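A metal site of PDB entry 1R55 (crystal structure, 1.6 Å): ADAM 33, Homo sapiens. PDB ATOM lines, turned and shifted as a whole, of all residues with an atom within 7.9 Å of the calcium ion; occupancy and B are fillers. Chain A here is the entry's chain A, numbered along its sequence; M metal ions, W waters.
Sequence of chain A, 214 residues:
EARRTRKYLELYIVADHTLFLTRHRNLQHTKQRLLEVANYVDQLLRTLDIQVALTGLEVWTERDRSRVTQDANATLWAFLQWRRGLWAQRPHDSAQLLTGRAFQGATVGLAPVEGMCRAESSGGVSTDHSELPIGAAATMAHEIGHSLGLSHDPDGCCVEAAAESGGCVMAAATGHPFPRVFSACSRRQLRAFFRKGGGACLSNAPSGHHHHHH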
ATOM      1  N   TYR A   8      21.715  29.932  30.922  1.00  0.00           N
ATOM      2  CA  TYR A   8      22.709  28.953  30.490  1.00  0.00           C
ATOM      3  C   TYR A   8      23.687  29.596  29.515  1.00  0.00           C
ATOM      4  O   TYR A   8      23.292  30.346  28.626  1.00  0.00           O
ATOM      5  CB  TYR A   8      22.038  27.775  29.772  1.00  0.00           C
ATOM      6  CG  TYR A   8      20.964  27.075  30.563  1.00  0.00           C
ATOM      7  CD1 TYR A   8      19.710  27.659  30.736  1.00  0.00           C
ATOM      8  CD2 TYR A   8      21.200  25.837  31.153  1.00  0.00           C
ATOM      9  CE1 TYR A   8      18.709  27.021  31.480  1.00  0.00           C
ATOM     10  CE2 TYR A   8      20.209  25.189  31.898  1.00  0.00           C
ATOM     11  CZ  TYR A   8      18.972  25.779  32.054  1.00  0.00           C
ATOM     12  OH  TYR A   8      18.013  25.142  32.799  1.00  0.00           O
ATOM     13  N   LEU A   9      24.968  29.279  29.684  1.00  0.00           N
ATOM     14  CA  LEU A   9      25.993  29.823  28.791  1.00  0.00           C
ATOM     15  C   LEU A   9      26.546  28.688  27.944  1.00  0.00           C
ATOM     16  O   LEU A   9      27.158  27.765  28.467  1.00  0.00           O
ATOM     17  CB  LEU A   9      27.136  30.455  29.589  1.00  0.00           C
ATOM     18  CG  LEU A   9      28.237  31.015  28.672  1.00  0.00           C
ATOM     19  CD1 LEU A   9      27.758  32.240  27.920  1.00  0.00           C
ATOM     20  CD2 LEU A   9      29.482  31.358  29.468  1.00  0.00           C
ATOM     21  N   GLU A  10      26.316  28.748  26.633  1.00  0.00           N
ATOM     22  CA  GLU A  10      26.832  27.733  25.738  1.00  0.00           C
ATOM     23  C   GLU A  10      28.244  28.184  25.379  1.00  0.00           C
ATOM     24  O   GLU A  10      28.446  29.120  24.601  1.00  0.00           O
ATOM     25  CB  GLU A  10      25.935  27.617  24.502  1.00  0.00           C
ATOM     26  CG  GLU A  10      24.573  27.047  24.874  1.00  0.00           C
ATOM     27  CD  GLU A  10      23.583  27.124  23.741  1.00  0.00           C
ATOM     28  OE1 GLU A  10      23.155  28.252  23.402  1.00  0.00           O
ATOM     29  OE2 GLU A  10      23.240  26.054  23.179  1.00  0.00           O
ATOM     30  N   LEU A  11      29.209  27.490  25.973  1.00  0.00           N
ATOM     31  CA  LEU A  11      30.625  27.804  25.825  1.00  0.00           C
ATOM     32  C   LEU A  11      31.384  26.921  24.854  1.00  0.00           C
ATOM     33  O   LEU A  11      31.238  25.698  24.857  1.00  0.00           O
ATOM     34  CB  LEU A  11      31.264  27.699  27.222  1.00  0.00           C
ATOM     35  CG  LEU A  11      32.775  27.910  27.285  1.00  0.00           C
ATOM     36  CD1 LEU A  11      33.135  29.352  26.972  1.00  0.00           C
ATOM     37  CD2 LEU A  11      33.292  27.551  28.681  1.00  0.00           C
ATOM     38  N   THR A  55      29.530  23.527  24.740  1.00  0.00           N
ATOM     39  CA  THR A  55      29.015  23.249  23.406  1.00  0.00           C
ATOM     40  C   THR A  55      30.008  22.563  22.480  1.00  0.00           C
ATOM     41  O   THR A  55      29.667  21.608  21.776  1.00  0.00           O
ATOM     42  CB  THR A  55      28.579  24.559  22.693  1.00  0.00           C
ATOM     43  OG1 THR A  55      27.543  25.192  23.441  1.00  0.00           O
ATOM     44  CG2 THR A  55      28.086  24.279  21.278  1.00  0.00           C
ATOM     45  N   PRO A  91      27.331  26.848  16.432  1.00  0.00           N
ATOM     46  CA  PRO A  91      26.701  27.866  17.278  1.00  0.00           C
ATOM     47  C   PRO A  91      27.077  27.719  18.741  1.00  0.00           C
ATOM     48  O   PRO A  91      27.227  26.601  19.252  1.00  0.00           O
ATOM     49  CB  PRO A  91      25.209  27.624  17.037  1.00  0.00           C
ATOM     50  CG  PRO A  91      25.165  27.124  15.643  1.00  0.00           C
ATOM     51  CD  PRO A  91      26.322  26.157  15.597  1.00  0.00           C
ATOM     52  N   HIS A  92      27.211  28.855  19.409  1.00  0.00           N
ATOM     53  CA  HIS A  92      27.561  28.920  20.815  1.00  0.00           C
ATOM     54  C   HIS A  92      27.296  30.355  21.266  1.00  0.00           C
ATOM     55  O   HIS A  92      27.061  31.230  20.430  1.00  0.00           O
ATOM     56  CB  HIS A  92      29.036  28.581  21.029  1.00  0.00           C
ATOM     57  CG  HIS A  92      29.969  29.449  20.223  1.00  0.00           C
ATOM     58  ND1 HIS A  92      30.315  29.166  18.926  1.00  0.00           N
ATOM     59  CD2 HIS A  92      30.553  30.637  20.520  1.00  0.00           C
ATOM     60  CE1 HIS A  92      31.063  30.146  18.453  1.00  0.00           C
ATOM     61  NE2 HIS A  92      31.222  31.051  19.398  1.00  0.00           N
ATOM     62  N   ASP A  93      27.360  30.610  22.567  1.00  0.00           N
ATOM     63  CA  ASP A  93      27.137  31.960  23.076  1.00  0.00           C
ATOM     64  C   ASP A  93      28.442  32.732  23.226  1.00  0.00           C
ATOM     65  O   ASP A  93      28.507  33.916  22.921  1.00  0.00           O
ATOM     66  CB  ASP A  93      26.457  31.909  24.446  1.00  0.00           C
ATOM     67  CG  ASP A  93      25.065  31.306  24.385  1.00  0.00           C
ATOM     68  OD1 ASP A  93      24.364  31.520  23.367  1.00  0.00           O
ATOM     69  OD2 ASP A  93      24.670  30.628  25.358  1.00  0.00           O
ATOM     70  N   SER A  94      29.486  32.039  23.671  1.00  0.00           N
ATOM     71  CA  SER A  94      30.792  32.654  23.889  1.00  0.00           C
ATOM     72  C   SER A  94      31.911  31.685  23.552  1.00  0.00           C
ATOM     73  O   SER A  94      31.846  30.512  23.896  1.00  0.00           O
ATOM     74  CB  SER A  94      30.903  33.066  25.367  1.00  0.00           C
ATOM     75  OG  SER A  94      32.155  33.661  25.668  1.00  0.00           O
ATOM     76  N   CYS A 117      26.899  37.658  23.246  1.00  0.00           N
ATOM     77  CA  CYS A 117      25.942  37.400  22.173  1.00  0.00           C
ATOM     78  C   CYS A 117      26.183  38.230  20.914  1.00  0.00           C
ATOM     79  O   CYS A 117      25.573  37.962  19.878  1.00  0.00           O
ATOM     80  CB  CYS A 117      24.501  37.641  22.655  1.00  0.00           C
ATOM     81  SG  CYS A 117      24.017  36.844  24.232  1.00  0.00           S
ATOM     82  N   GLY A 199      22.758  40.129  27.105  1.00  0.00           N
ATOM     83  CA  GLY A 199      22.867  38.674  27.180  1.00  0.00           C
ATOM     84  C   GLY A 199      21.616  37.880  26.874  1.00  0.00           C
ATOM     85  O   GLY A 199      21.347  36.868  27.508  1.00  0.00           O
ATOM     86  N   ALA A 200      20.866  38.326  25.873  1.00  0.00           N
ATOM     87  CA  ALA A 200      19.634  37.646  25.496  1.00  0.00           C
ATOM     88  C   ALA A 200      19.827  36.191  25.090  1.00  0.00           C
ATOM     89  O   ALA A 200      18.916  35.380  25.232  1.00  0.00           O
ATOM     90  CB  ALA A 200      18.932  38.417  24.387  1.00  0.00           C
ATOM     91  N   CYS A 201      21.014  35.854  24.592  1.00  0.00           N
ATOM     92  CA  CYS A 201      21.271  34.492  24.142  1.00  0.00           C
ATOM     93  C   CYS A 201      21.490  33.454  25.245  1.00  0.00           C
ATOM     94  O   CYS A 201      21.638  32.263  24.964  1.00  0.00           O
ATOM     95  CB  CYS A 201      22.461  34.464  23.165  1.00  0.00           C
ATOM     96  SG  CYS A 201      24.103  34.841  23.854  1.00  0.00           S
ATOM     97  N   LEU A 202      21.510  33.893  26.502  1.00  0.00           N
ATOM     98  CA  LEU A 202      21.693  32.961  27.614  1.00  0.00           C
ATOM     99  C   LEU A 202      20.359  32.395  28.106  1.00  0.00           C
ATOM    100  O   LEU A 202      20.320  31.685  29.110  1.00  0.00           O
ATOM    101  CB  LEU A 202      22.372  33.658  28.795  1.00  0.00           C
ATOM    102  CG  LEU A 202      23.900  33.716  28.685  1.00  0.00           C
ATOM    103  CD1 LEU A 202      24.327  34.736  27.667  1.00  0.00           C
ATOM    104  CD2 LEU A 202      24.513  34.044  30.035  1.00  0.00           C
ATOM    105  N   SER A 203      19.280  32.686  27.393  1.00  0.00           N
ATOM    106  CA  SER A 203      17.960  32.220  27.798  1.00  0.00           C
ATOM    107  C   SER A 203      17.581  30.784  27.451  1.00  0.00           C
ATOM    108  O   SER A 203      16.688  30.218  28.072  1.00  0.00           O
ATOM    109  CB  SER A 203      16.889  33.161  27.243  1.00  0.00           C
ATOM    110  OG  SER A 203      16.963  34.434  27.852  1.00  0.00           O
ATOM    111  N   ASN A 204      18.244  30.184  26.461  1.00  0.00           N
ATOM    112  CA  ASN A 204      17.889  28.831  26.072  1.00  0.00           C
ATOM    113  C   ASN A 204      18.642  27.719  26.789  1.00  0.00           C
ATOM    114  O   ASN A 204      19.856  27.799  27.006  1.00  0.00           O
ATOM    115  CB  ASN A 204      18.055  28.636  24.558  1.00  0.00           C
ATOM    116  CG  ASN A 204      19.491  28.744  24.092  1.00  0.00           C
ATOM    117  OD1 ASN A 204      20.127  29.785  24.237  1.00  0.00           O
ATOM    118  ND2 ASN A 204      20.007  27.665  23.516  1.00  0.00           N
ATOM    119  N   ALA A 205      17.912  26.681  27.168  1.00  0.00           N
ATOM    120  CA  ALA A 205      18.497  25.527  27.831  1.00  0.00           C
ATOM    121  C   ALA A 205      19.079  24.668  26.713  1.00  0.00           C
ATOM    122  O   ALA A 205      18.357  24.272  25.785  1.00  0.00           O
ATOM    123  CB  ALA A 205      17.423  24.755  28.590  1.00  0.00           C
ATOM    124  N   PRO A 206      20.387  24.382  26.770  1.00  0.00           N
ATOM    125  CA  PRO A 206      21.031  23.569  25.731  1.00  0.00           C
ATOM    126  C   PRO A 206      20.324  22.250  25.460  1.00  0.00           C
ATOM    127  O   PRO A 206      19.803  21.601  26.369  1.00  0.00           O
ATOM    128  CB  PRO A 206      22.446  23.377  26.280  1.00  0.00           C
ATOM    129  CG  PRO A 206      22.259  23.479  27.763  1.00  0.00           C
ATOM    130  CD  PRO A 206      21.302  24.631  27.888  1.00  0.00           C
HETATM  131 CA    CA M   1      22.428  30.295  24.202  1.00  0.00          CA
HETATM  132  O   HOH W   1      22.007  29.347  26.472  1.00  0.00           O
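The side-chain sulfur of Cys 201 forms a disulfide with the side-chain sulfur of Cys 117 (2.0 Å). The backbone carbonyl oxygen (O) of Glu 10 sits at hydrogen-bond distance from the backbone NH (N) of Ser 94.
Of the 18 residues printed, 4 come within 4 Å of the calcium ion.
The calcium ion is bound by the backbone carbonyl oxygen (O) of Cys 201 (2.3 Å), the side-chain carboxylate (OE1) of Glu 10 (2.3 Å), the side-chain amide oxygen (OD1) of Asn 204 (2.4 Å), the side-chain carboxylate (OD1) of Asp 93 (2.4 Å), water W1 (2.5 Å) and the side-chain carboxylate (OD2) of Asp 93 (2.5 Å).
Water W1 bridges the backbone carbonyl oxygen (O) of Tyr 8 (2.7 Å) and the backbone carbonyl oxygen (O) of Asn 204 (2.7 Å).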
